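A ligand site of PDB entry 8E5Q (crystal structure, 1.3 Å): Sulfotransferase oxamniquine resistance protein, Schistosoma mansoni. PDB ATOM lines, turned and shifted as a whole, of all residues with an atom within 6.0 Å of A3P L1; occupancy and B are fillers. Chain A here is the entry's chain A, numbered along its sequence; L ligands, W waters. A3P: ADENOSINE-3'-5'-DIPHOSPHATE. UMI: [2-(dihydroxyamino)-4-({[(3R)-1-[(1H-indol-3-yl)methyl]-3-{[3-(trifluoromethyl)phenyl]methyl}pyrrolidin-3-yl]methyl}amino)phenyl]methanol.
NE of Arg 19 lies within hydrogen-bond range of OG of Ser 125, at 2.7 Å. A ring nitrogen (NE2) of His 39 is in hydrogen-bond range of the side-chain carboxylate (OD2) of Asp 93. The side-chain hydroxyl (OG) of Ser 231 sits close to the backbone NH (N) of His 233 (3.5 Å). O of Arg 19 is in hydrogen-bond range of NH1 of Arg 117 (2.9 Å). The backbone carbonyl oxygen (O) of Leu 17 is in hydrogen-bond range of the side-chain hydroxyl (OG1) of Thr 20, 2.6 Å away. The side-chain hydroxyl of Ser 24 lies within hydrogen-bond range of the backbone carbonyl oxygen of Pro 227, 3.1 Å away. OG1 of Thr 22 lies within hydrogen-bond range of NE2 of His 39 (3.1 Å). The side-chain hydroxyl (OG) of Ser 24 sits at hydrogen-bond distance from the backbone NH (N) of Val 229 (3.1 Å).
Water W5 lies within hydrogen-bond range of an oxygen (O6P) of A3P L1 (2.7 Å), the backbone NH (N) of Ser 24 (2.9 Å), the backbone carbonyl oxygen (O) of Val 229 (3.0 Å) and the backbone NH (N) of Lys 23 (3.4 Å). Water W9 lies within hydrogen-bond range of O2P of A3P L1, O of Asp 121 and ND1 of His 124. Water W1 bridges O2' of A3P L1 and SG of Cys 228. Water W3 lies within hydrogen-bond range of O3P of A3P L1 (2.8 Å), N of His 233 (3.1 Å) and N of His 232 (3.2 Å). Water W7 bridges O of Tyr 226 and N6 of A3P L1. Water W8 bridges N of Gly 206 (2.8 Å) and N6 of A3P L1 (3.4 Å).
Merely in contact with A3P L1: Pro 18 (3.97 Å), Asp 93 (3.9 Å), Leu 205 (3.5 Å), Tyr 226 (3.998 Å), Val 229 (3.5 Å) and Ser 231 (3.3 Å). Hydrophobic or aromatic side chains within 4 Å of A3P L1: Leu 205, Tyr 226 and His 232. 18 residues have an atom within 4 Å of A3P L1: Pro 18, Arg 19, Thr 20, Gly 21, Thr 22, Lys 23, Ser 24, Asp 93, Arg 117, Ser 125, Leu 205, Tyr 226, Pro 227, Cys 228, Val 229, Asn 230, Ser 231 and His 232. The nearest printed residue that does not touch A3P L1 is Gly 206 (4.3 Å).
O3P of A3P L1 lies within hydrogen-bond range of N of His 232, 3.1 Å away. N of Thr 20 sits at hydrogen-bond distance from O5P of A3P L1, 3.2 Å away. The backbone NH of Lys 23 is in hydrogen-bond range of an oxygen (O6P) of A3P L1, 2.8 Å away. An oxygen (O5P) of A3P L1 sits at hydrogen-bond distance from the side-chain hydroxyl (OG1) of Thr 22, at 2.6 Å. An oxygen (O2P) of A3P L1 lies within salt-bridge range of the guanidinium group of Arg 117 (2.8 Å). OG of Ser 24 lies within hydrogen-bond range of N7 of A3P L1. O5' of A3P L1 sits at hydrogen-bond distance from N of Gly 21 (2.9 Å). The side-chain amide nitrogen (ND2) of Asn 230 is in hydrogen-bond range of an oxygen (O6P) of A3P L1, 3.0 Å away. NH1 of Arg 19 is in salt-bridge range of O4P of A3P L1 (2.8 Å). The backbone NH (N) of Arg 19 is in hydrogen-bond range of an oxygen (O5P) of A3P L1 (3.0 Å). An oxygen (O9) of UMI L2 lies within hydrogen-bond range of the side-chain carboxylate of Asp 93 (2.5 Å). O5P of A3P L1 sits at hydrogen-bond distance from N of Thr 22 (2.6 Å). N1 of A3P L1 lies close to SG of Cys 228, at 3.6 Å. An oxygen (O1P) of A3P L1 is in hydrogen-bond range of the side-chain hydroxyl of Ser 125. N6 of A3P L1 is in hydrogen-bond range of O of Pro 227, at 2.9 Å.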
ATOM      1  N   LEU A  17      29.602  13.517  -4.417  1.00  0.00           N
ATOM      2  CA  LEU A  17      30.791  13.993  -5.117  1.00  0.00           C
ATOM      3  C   LEU A  17      30.424  14.513  -6.504  1.00  0.00           C
ATOM      4  O   LEU A  17      29.359  14.178  -7.034  1.00  0.00           O
ATOM      5  CB  LEU A  17      31.777  12.835  -5.241  1.00  0.00           C
ATOM      6  CG  LEU A  17      32.356  12.443  -3.868  1.00  0.00           C
ATOM      7  CD1 LEU A  17      33.033  11.092  -3.977  1.00  0.00           C
ATOM      8  CD2 LEU A  17      33.350  13.480  -3.343  1.00  0.00           C
ATOM      9  N   PRO A  18      31.275  15.343  -7.105  1.00  0.00           N
ATOM     10  CA  PRO A  18      31.014  15.767  -8.490  1.00  0.00           C
ATOM     11  C   PRO A  18      30.858  14.558  -9.406  1.00  0.00           C
ATOM     12  O   PRO A  18      31.485  13.518  -9.189  1.00  0.00           O
ATOM     13  CB  PRO A  18      32.265  16.569  -8.862  1.00  0.00           C
ATOM     14  CG  PRO A  18      33.307  16.138  -7.867  1.00  0.00           C
ATOM     15  CD  PRO A  18      32.558  15.860  -6.614  1.00  0.00           C
ATOM     16  N   ARG A  19      30.005  14.718 -10.428  1.00  0.00           N
ATOM     17  CA  ARG A  19      29.740  13.691 -11.433  1.00  0.00           C
ATOM     18  C   ARG A  19      28.891  12.544 -10.898  1.00  0.00           C
ATOM     19  O   ARG A  19      28.936  11.425 -11.421  1.00  0.00           O
ATOM     20  CB  ARG A  19      31.000  13.208 -12.169  1.00  0.00           C
ATOM     21  CG  ARG A  19      31.926  14.311 -12.688  1.00  0.00           C
ATOM     22  CD  ARG A  19      31.175  15.397 -13.456  1.00  0.00           C
ATOM     23  NE  ARG A  19      30.604  14.843 -14.686  1.00  0.00           N
ATOM     24  CZ  ARG A  19      29.795  15.483 -15.508  1.00  0.00           C
ATOM     25  NH1 ARG A  19      29.402  16.721 -15.257  1.00  0.00           N
ATOM     26  NH2 ARG A  19      29.393  14.883 -16.642  1.00  0.00           N
ATOM     27  N   THR A  20      28.072  12.796  -9.883  1.00  0.00           N
ATOM     28  CA  THR A  20      27.138  11.801  -9.375  1.00  0.00           C
ATOM     29  C   THR A  20      25.683  12.218  -9.568  1.00  0.00           C
ATOM     30  O   THR A  20      24.795  11.640  -8.946  1.00  0.00           O
ATOM     31  CB  THR A  20      27.403  11.490  -7.887  1.00  0.00           C
ATOM     32  OG1 THR A  20      27.242  12.683  -7.109  1.00  0.00           O
ATOM     33  CG2 THR A  20      28.802  10.957  -7.664  1.00  0.00           C
ATOM     34  N   GLY A  21      25.433  13.249 -10.374  1.00  0.00           N
ATOM     35  CA  GLY A  21      24.097  13.785 -10.542  1.00  0.00           C
ATOM     36  C   GLY A  21      23.812  15.042  -9.738  1.00  0.00           C
ATOM     37  O   GLY A  21      22.633  15.317  -9.448  1.00  0.00           O
ATOM     38  N   THR A  22      24.841  15.807  -9.374  1.00  0.00           N
ATOM     39  CA  THR A  22      24.627  16.959  -8.505  1.00  0.00           C
ATOM     40  C   THR A  22      23.924  18.096  -9.222  1.00  0.00           C
ATOM     41  O   THR A  22      23.172  18.842  -8.583  1.00  0.00           O
ATOM     42  CB  THR A  22      25.952  17.465  -7.915  1.00  0.00           C
ATOM     43  OG1 THR A  22      26.817  17.904  -8.977  1.00  0.00           O
ATOM     44  CG2 THR A  22      26.643  16.393  -7.071  1.00  0.00           C
ATOM     45  N   LYS A  23      24.143  18.289 -10.524  1.00  0.00           N
ATOM     46  CA  LYS A  23      23.467  19.387 -11.208  1.00  0.00           C
ATOM     47  C   LYS A  23      21.994  19.066 -11.401  1.00  0.00           C
ATOM     48  O   LYS A  23      21.134  19.937 -11.251  1.00  0.00           O
ATOM     49  CB  LYS A  23      24.173  19.724 -12.521  1.00  0.00           C
ATOM     50  CG  LYS A  23      23.552  20.851 -13.335  1.00  0.00           C
ATOM     51  CD  LYS A  23      23.609  22.182 -12.615  1.00  0.00           C
ATOM     52  CE  LYS A  23      23.387  23.332 -13.589  1.00  0.00           C
ATOM     53  NZ  LYS A  23      21.980  23.451 -14.059  1.00  0.00           N
ATOM     54  N   SER A  24      21.677  17.805 -11.708  1.00  0.00           N
ATOM     55  CA  SER A  24      20.278  17.397 -11.748  1.00  0.00           C
ATOM     56  C   SER A  24      19.610  17.597 -10.396  1.00  0.00           C
ATOM     57  O   SER A  24      18.459  18.006 -10.320  1.00  0.00           O
ATOM     58  CB  SER A  24      20.161  15.947 -12.187  1.00  0.00           C
ATOM     59  OG  SER A  24      20.484  15.818 -13.568  1.00  0.00           O
ATOM     60  N   HIS A  39      26.211  25.370  -6.235  1.00  0.00           N
ATOM     61  CA  HIS A  39      26.791  24.296  -7.031  1.00  0.00           C
ATOM     62  C   HIS A  39      28.005  24.985  -7.623  1.00  0.00           C
ATOM     63  O   HIS A  39      28.061  26.213  -7.614  1.00  0.00           O
ATOM     64  CB  HIS A  39      25.831  23.851  -8.117  1.00  0.00           C
ATOM     65  CG  HIS A  39      26.345  22.747  -8.982  1.00  0.00           C
ATOM     66  ND1 HIS A  39      27.192  22.965 -10.055  1.00  0.00           N
ATOM     67  CD2 HIS A  39      26.111  21.408  -8.960  1.00  0.00           C
ATOM     68  CE1 HIS A  39      27.472  21.815 -10.640  1.00  0.00           C
ATOM     69  NE2 HIS A  39      26.822  20.859 -10.001  1.00  0.00           N
ATOM     70  N   ASP A  93      27.670  19.662  -4.834  1.00  0.00           N
ATOM     71  CA  ASP A  93      28.946  19.575  -5.547  1.00  0.00           C
ATOM     72  C   ASP A  93      30.134  20.166  -4.780  1.00  0.00           C
ATOM     73  O   ASP A  93      29.999  20.667  -3.660  1.00  0.00           O
ATOM     74  CB  ASP A  93      28.790  20.258  -6.905  1.00  0.00           C
ATOM     75  CG  ASP A  93      29.355  19.432  -8.012  1.00  0.00           C
ATOM     76  OD1 ASP A  93      30.541  19.062  -7.920  1.00  0.00           O
ATOM     77  OD2 ASP A  93      28.630  19.187  -9.005  1.00  0.00           O
ATOM     78  N   ARG A 117      26.676   6.507  -7.653  1.00  0.00           N
ATOM     79  CA  ARG A 117      26.562   5.757  -8.904  1.00  0.00           C
ATOM     80  C   ARG A 117      27.722   4.774  -8.964  1.00  0.00           C
ATOM     81  O   ARG A 117      28.646   4.798  -8.136  1.00  0.00           O
ATOM     82  CB  ARG A 117      26.640   6.693 -10.112  1.00  0.00           C
ATOM     83  CG  ARG A 117      28.029   7.256 -10.325  1.00  0.00           C
ATOM     84  CD  ARG A 117      28.054   8.345 -11.392  1.00  0.00           C
ATOM     85  NE  ARG A 117      27.722   7.838 -12.725  1.00  0.00           N
ATOM     86  CZ  ARG A 117      27.839   8.574 -13.822  1.00  0.00           C
ATOM     87  NH1 ARG A 117      28.347   9.787 -13.792  1.00  0.00           N
ATOM     88  NH2 ARG A 117      27.463   8.050 -14.987  1.00  0.00           N
ATOM     89  N   ASP A 121      31.775   4.236 -13.810  1.00  0.00           N
ATOM     90  CA  ASP A 121      31.101   5.316 -14.509  1.00  0.00           C
ATOM     91  C   ASP A 121      31.458   6.666 -13.913  1.00  0.00           C
ATOM     92  O   ASP A 121      31.700   7.635 -14.651  1.00  0.00           O
ATOM     93  CB  ASP A 121      29.580   5.168 -14.515  1.00  0.00           C
ATOM     94  CG  ASP A 121      29.106   3.837 -15.092  1.00  0.00           C
ATOM     95  OD1 ASP A 121      29.812   3.246 -15.945  1.00  0.00           O
ATOM     96  OD2 ASP A 121      27.932   3.464 -14.837  1.00  0.00           O
ATOM     97  N   HIS A 124      35.152   7.704 -14.937  1.00  0.00           N
ATOM     98  CA  HIS A 124      35.249   8.168 -16.322  1.00  0.00           C
ATOM     99  C   HIS A 124      34.702   9.587 -16.423  1.00  0.00           C
ATOM    100  O   HIS A 124      35.280  10.451 -17.092  1.00  0.00           O
ATOM    101  CB  HIS A 124      34.363   7.323 -17.207  1.00  0.00           C
ATOM    102  CG  HIS A 124      34.256   7.915 -18.568  1.00  0.00           C
ATOM    103  ND1 HIS A 124      33.067   8.369 -19.089  1.00  0.00           N
ATOM    104  CD2 HIS A 124      35.187   8.081 -19.528  1.00  0.00           C
ATOM    105  CE1 HIS A 124      33.287   8.853 -20.306  1.00  0.00           C
ATOM    106  NE2 HIS A 124      34.572   8.691 -20.591  1.00  0.00           N
ATOM    107  N   SER A 125      33.538   9.811 -15.805  1.00  0.00           N
ATOM    108  CA  SER A 125      32.892  11.112 -15.858  1.00  0.00           C
ATOM    109  C   SER A 125      33.781  12.179 -15.233  1.00  0.00           C
ATOM    110  O   SER A 125      33.952  13.272 -15.793  1.00  0.00           O
ATOM    111  CB  SER A 125      31.530  11.006 -15.158  1.00  0.00           C
ATOM    112  OG  SER A 125      30.748  12.172 -15.305  1.00  0.00           O
ATOM    113  N   VAL A 129      35.532  15.463 -17.361  1.00  0.00           N
ATOM    114  CA  VAL A 129      34.918  16.750 -17.096  1.00  0.00           C
ATOM    115  C   VAL A 129      35.670  17.556 -16.051  1.00  0.00           C
ATOM    116  O   VAL A 129      35.893  18.749 -16.241  1.00  0.00           O
ATOM    117  CB  VAL A 129      33.424  16.607 -16.716  1.00  0.00           C
ATOM    118  CG1 VAL A 129      32.820  17.963 -16.345  1.00  0.00           C
ATOM    119  CG2 VAL A 129      32.627  15.924 -17.829  1.00  0.00           C
ATOM    120  N   VAL A 130      36.088  16.927 -14.964  1.00  0.00           N
ATOM    121  CA  VAL A 130      36.543  17.641 -13.765  1.00  0.00           C
ATOM    122  C   VAL A 130      38.051  17.565 -13.603  1.00  0.00           C
ATOM    123  O   VAL A 130      38.703  18.578 -13.331  1.00  0.00           O
ATOM    124  CB  VAL A 130      35.831  17.102 -12.509  1.00  0.00           C
ATOM    125  CG1 VAL A 130      36.326  17.828 -11.239  1.00  0.00           C
ATOM    126  CG2 VAL A 130      34.351  17.236 -12.665  1.00  0.00           C
ATOM    127  N   LEU A 205      21.509   7.231  -9.410  1.00  0.00           N
ATOM    128  CA  LEU A 205      21.064   7.730 -10.702  1.00  0.00           C
ATOM    129  C   LEU A 205      19.938   6.864 -11.221  1.00  0.00           C
ATOM    130  O   LEU A 205      20.018   5.629 -11.189  1.00  0.00           O
ATOM    131  CB  LEU A 205      22.228   7.712 -11.711  1.00  0.00           C
ATOM    132  CG  LEU A 205      23.318   8.786 -11.587  1.00  0.00           C
ATOM    133  CD1 LEU A 205      24.360   8.632 -12.700  1.00  0.00           C
ATOM    134  CD2 LEU A 205      22.726  10.203 -11.575  1.00  0.00           C
ATOM    135  N   GLY A 206      18.857   7.507 -11.674  1.00  0.00           N
ATOM    136  CA  GLY A 206      17.669   6.823 -12.123  1.00  0.00           C
ATOM    137  C   GLY A 206      16.550   6.718 -11.097  1.00  0.00           C
ATOM    138  O   GLY A 206      15.467   6.235 -11.440  1.00  0.00           O
ATOM    139  N   TYR A 226      12.246  13.784 -13.736  1.00  0.00           N
ATOM    140  CA  TYR A 226      13.350  14.197 -12.904  1.00  0.00           C
ATOM    141  C   TYR A 226      14.472  14.719 -13.797  1.00  0.00           C
ATOM    142  O   TYR A 226      14.705  14.173 -14.889  1.00  0.00           O
ATOM    143  CB  TYR A 226      13.851  13.012 -12.080  1.00  0.00           C
ATOM    144  CG  TYR A 226      14.891  13.399 -11.078  1.00  0.00           C
ATOM    145  CD1 TYR A 226      14.536  13.930  -9.854  1.00  0.00           C
ATOM    146  CD2 TYR A 226      16.243  13.271 -11.378  1.00  0.00           C
ATOM    147  CE1 TYR A 226      15.496  14.298  -8.934  1.00  0.00           C
ATOM    148  CE2 TYR A 226      17.210  13.640 -10.479  1.00  0.00           C
ATOM    149  CZ  TYR A 226      16.823  14.144  -9.260  1.00  0.00           C
ATOM    150  OH  TYR A 226      17.775  14.514  -8.351  1.00  0.00           O
ATOM    151  N   PRO A 227      15.172  15.789 -13.404  1.00  0.00           N
ATOM    152  CA  PRO A 227      16.208  16.359 -14.274  1.00  0.00           C
ATOM    153  C   PRO A 227      17.272  15.346 -14.674  1.00  0.00           C
ATOM    154  O   PRO A 227      17.677  14.486 -13.887  1.00  0.00           O
ATOM    155  CB  PRO A 227      16.803  17.502 -13.428  1.00  0.00           C
ATOM    156  CG  PRO A 227      15.682  17.887 -12.531  1.00  0.00           C
ATOM    157  CD  PRO A 227      14.948  16.614 -12.203  1.00  0.00           C
ATOM    158  N   CYS A 228      17.716  15.452 -15.917  1.00  0.00           N
ATOM    159  CA  CYS A 228      18.789  14.658 -16.514  1.00  0.00           C
ATOM    160  C   CYS A 228      19.693  15.598 -17.300  1.00  0.00           C
ATOM    161  O   CYS A 228      19.579  15.712 -18.515  1.00  0.00           O
ATOM    162  CB  CYS A 228      18.220  13.594 -17.433  1.00  0.00           C
ATOM    163  SG  CYS A 228      19.381  12.295 -17.840  1.00  0.00           S
ATOM    164  N   VAL A 229      20.618  16.240 -16.594  1.00  0.00           N
ATOM    165  CA  VAL A 229      21.424  17.293 -17.178  1.00  0.00           C
ATOM    166  C   VAL A 229      22.885  17.018 -16.858  1.00  0.00           C
ATOM    167  O   VAL A 229      23.213  16.195 -16.013  1.00  0.00           O
ATOM    168  CB  VAL A 229      20.990  18.691 -16.663  1.00  0.00           C
ATOM    169  CG1 VAL A 229      19.568  19.017 -17.130  1.00  0.00           C
ATOM    170  CG2 VAL A 229      21.118  18.797 -15.134  1.00  0.00           C
ATOM    171  N   ASN A 230      23.770  17.732 -17.571  1.00  0.00           N
ATOM    172  CA  ASN A 230      25.188  17.762 -17.256  1.00  0.00           C
ATOM    173  C   ASN A 230      25.912  16.475 -17.651  1.00  0.00           C
ATOM    174  O   ASN A 230      26.883  16.078 -17.013  1.00  0.00           O
ATOM    175  CB  ASN A 230      25.422  18.132 -15.786  1.00  0.00           C
ATOM    176  CG  ASN A 230      26.688  18.908 -15.567  1.00  0.00           C
ATOM    177  OD1 ASN A 230      27.157  19.608 -16.467  1.00  0.00           O
ATOM    178  ND2 ASN A 230      27.231  18.843 -14.361  1.00  0.00           N
ATOM    179  N   SER A 231      25.483  15.807 -18.726  1.00  0.00           N
ATOM    180  CA  SER A 231      26.149  14.576 -19.129  1.00  0.00           C
ATOM    181  C   SER A 231      27.552  14.881 -19.675  1.00  0.00           C
ATOM    182  O   SER A 231      27.841  15.984 -20.126  1.00  0.00           O
ATOM    183  CB  SER A 231      25.340  13.872 -20.206  1.00  0.00           C
ATOM    184  OG  SER A 231      25.396  14.603 -21.419  1.00  0.00           O
ATOM    185  N   HIS A 232      28.428  13.876 -19.630  1.00  0.00           N
ATOM    186  CA  HIS A 232      29.746  14.078 -20.234  1.00  0.00           C
ATOM    187  C   HIS A 232      29.646  14.335 -21.729  1.00  0.00           C
ATOM    188  O   HIS A 232      30.469  15.058 -22.281  1.00  0.00           O
ATOM    189  CB  HIS A 232      30.732  12.958 -19.870  1.00  0.00           C
ATOM    190  CG  HIS A 232      30.507  11.657 -20.587  1.00  0.00           C
ATOM    191  ND1 HIS A 232      30.787  11.469 -21.922  1.00  0.00           N
ATOM    192  CD2 HIS A 232      30.029  10.470 -20.133  1.00  0.00           C
ATOM    193  CE1 HIS A 232      30.512  10.220 -22.261  1.00  0.00           C
ATOM    194  NE2 HIS A 232      30.051   9.592 -21.195  1.00  0.00           N
ATOM    195  N   HIS A 233      28.630  13.775 -22.390  1.00  0.00           N
ATOM    196  CA  HIS A 233      28.451  14.074 -23.807  1.00  0.00           C
ATOM    197  C   HIS A 233      28.196  15.561 -24.014  1.00  0.00           C
ATOM    198  O   HIS A 233      28.783  16.183 -24.905  1.00  0.00           O
ATOM    199  CB  HIS A 233      27.312  13.200 -24.345  1.00  0.00           C
ATOM    200  CG  HIS A 233      27.145  13.268 -25.821  1.00  0.00           C
ATOM    201  ND1 HIS A 233      27.554  12.253 -26.665  1.00  0.00           N
ATOM    202  CD2 HIS A 233      26.586  14.207 -26.619  1.00  0.00           C
ATOM    203  CE1 HIS A 233      27.275  12.578 -27.918  1.00  0.00           C
ATOM    204  NE2 HIS A 233      26.694  13.763 -27.913  1.00  0.00           N
HETATM  205  P1  A3P L   1      27.907  11.107 -17.294  1.00  0.00           P
HETATM  206  O1P A3P L   1      29.191  12.034 -17.304  1.00  0.00           O
HETATM  207  O2P A3P L   1      28.315   9.607 -17.178  1.00  0.00           O
HETATM  208  O3P A3P L   1      27.027  11.426 -18.446  1.00  0.00           O
HETATM  209  P2  A3P L   1      27.104  16.118 -12.004  1.00  0.00           P
HETATM  210  O4P A3P L   1      28.455  16.698 -12.599  1.00  0.00           O
HETATM  211  O5P A3P L   1      27.249  15.840 -10.449  1.00  0.00           O
HETATM  212  O6P A3P L   1      25.969  17.021 -12.306  1.00  0.00           O
HETATM  213  O5' A3P L   1      26.750  14.644 -12.566  1.00  0.00           O
HETATM  214  C5' A3P L   1      26.560  14.510 -13.986  1.00  0.00           C
HETATM  215  C4' A3P L   1      26.481  13.023 -14.287  1.00  0.00           C
HETATM  216  O4' A3P L   1      25.212  12.492 -13.816  1.00  0.00           O
HETATM  217  C3' A3P L   1      26.523  12.676 -15.779  1.00  0.00           C
HETATM  218  O3' A3P L   1      27.109  11.359 -15.882  1.00  0.00           O
HETATM  219  C2' A3P L   1      25.039  12.663 -16.134  1.00  0.00           C
HETATM  220  O2' A3P L   1      24.738  11.967 -17.339  1.00  0.00           O
HETATM  221  C1' A3P L   1      24.503  11.937 -14.908  1.00  0.00           C
HETATM  222  N9  A3P L   1      23.079  12.130 -14.682  1.00  0.00           N
HETATM  223  C8  A3P L   1      22.488  13.277 -14.219  1.00  0.00           C
HETATM  224  N7  A3P L   1      21.190  13.202 -14.108  1.00  0.00           N
HETATM  225  C5  A3P L   1      20.899  11.921 -14.522  1.00  0.00           C
HETATM  226  C6  A3P L   1      19.678  11.215 -14.623  1.00  0.00           C
HETATM  227  N6  A3P L   1      18.491  11.747 -14.312  1.00  0.00           N
HETATM  228  N1  A3P L   1      19.731   9.937 -15.080  1.00  0.00           N
HETATM  229  C2  A3P L   1      20.925   9.410 -15.402  1.00  0.00           C
HETATM  230  N3  A3P L   1      22.129   9.978 -15.336  1.00  0.00           N
HETATM  231  C4  A3P L   1      22.050  11.249 -14.889  1.00  0.00           C
HETATM  232  C1  UMI L   2      33.447  22.108 -10.049  1.00  0.00           C
HETATM  233  C10 UMI L   2      33.299  22.146 -16.075  1.00  0.00           C
HETATM  234  C11 UMI L   2      37.527  22.423 -14.375  1.00  0.00           C
HETATM  235  C12 UMI L   2      32.272  23.015 -14.299  1.00  0.00           C
HETATM  236  C14 UMI L   2      37.649  21.567 -15.613  1.00  0.00           C
HETATM  237  C15 UMI L   2      36.580  22.042 -16.571  1.00  0.00           C
HETATM  238  C16 UMI L   2      33.295  23.976 -14.709  1.00  0.00           C
HETATM  239  C17 UMI L   2      36.492  23.484 -14.715  1.00  0.00           C
HETATM  240  C18 UMI L   2      31.523  23.322 -13.202  1.00  0.00           C
HETATM  241  C19 UMI L   2      31.712  24.537 -12.587  1.00  0.00           C
HETATM  242  C2  UMI L   2      32.725  21.199 -10.823  1.00  0.00           C
HETATM  243  C20 UMI L   2      32.693  25.433 -12.971  1.00  0.00           C
HETATM  244  C21 UMI L   2      33.508  25.168 -14.056  1.00  0.00           C
HETATM  245  C22 UMI L   2      38.819  23.142 -13.982  1.00  0.00           C
HETATM  246  C23 UMI L   2      39.980  22.208 -13.722  1.00  0.00           C
HETATM  247  C24 UMI L   2      40.312  21.854 -12.415  1.00  0.00           C
HETATM  248  C25 UMI L   2      41.384  20.999 -12.173  1.00  0.00           C
HETATM  249  C26 UMI L   2      42.130  20.507 -13.239  1.00  0.00           C
HETATM  250  C27 UMI L   2      41.798  20.865 -14.536  1.00  0.00           C
HETATM  251  C28 UMI L   2      40.740  21.721 -14.778  1.00  0.00           C
HETATM  252  C29 UMI L   2      42.600  20.346 -15.695  1.00  0.00           C
HETATM  253  C3  UMI L   2      33.193  20.668 -11.998  1.00  0.00           C
HETATM  254  C30 UMI L   2      37.023  21.536 -13.237  1.00  0.00           C
HETATM  255  C4  UMI L   2      34.424  21.072 -12.478  1.00  0.00           C
HETATM  256  C5  UMI L   2      35.184  21.969 -11.740  1.00  0.00           C
HETATM  257  C6  UMI L   2      34.704  22.477 -10.537  1.00  0.00           C
HETATM  258  C7  UMI L   2      31.398  20.713 -10.347  1.00  0.00           C
HETATM  259  C8  UMI L   2      35.067  23.936 -16.686  1.00  0.00           C
HETATM  260  C9  UMI L   2      33.940  23.358 -15.881  1.00  0.00           C
HETATM  261  F30 UMI L   2      43.653  21.108 -15.860  1.00  0.00           F
HETATM  262  F31 UMI L   2      42.982  19.112 -15.417  1.00  0.00           F
HETATM  263  F32 UMI L   2      41.861  20.360 -16.784  1.00  0.00           F
HETATM  264  N11 UMI L   2      32.328  21.970 -15.135  1.00  0.00           N
HETATM  265  N12 UMI L   2      36.390  22.343 -12.212  1.00  0.00           N
HETATM  266  N16 UMI L   2      36.355  23.441 -16.179  1.00  0.00           N
HETATM  267  N8  UMI L   2      32.383  19.774 -12.729  1.00  0.00           N
HETATM  268  O10 UMI L   2      31.844  18.603 -12.190  1.00  0.00           O
HETATM  269  O11 UMI L   2      32.082  20.060 -14.057  1.00  0.00           O
HETATM  270  O9  UMI L   2      31.435  21.137  -8.986  1.00  0.00           O
HETATM  271  O   HOH W   1      22.608  11.808 -19.043  1.00  0.00           O
HETATM  272  O   HOH W   2      26.082   8.233 -18.440  1.00  0.00           O
HETATM  273  O   HOH W   3      27.125  11.365 -21.223  1.00  0.00           O
HETATM  274  O   HOH W   4      23.861   8.159 -16.749  1.00  0.00           O
HETATM  275  O   HOH W   5      23.558  16.139 -13.072  1.00  0.00           O
HETATM  276  O   HOH W   6      17.562   8.187 -15.472  1.00  0.00           O
HETATM  277  O   HOH W   7      15.487  11.553 -15.246  1.00  0.00           O
HETATM  278  O   HOH W   8      18.589  10.232 -11.296  1.00  0.00           O
HETATM  279  O   HOH W   9      30.604   8.117 -17.257  1.00  0.00           O
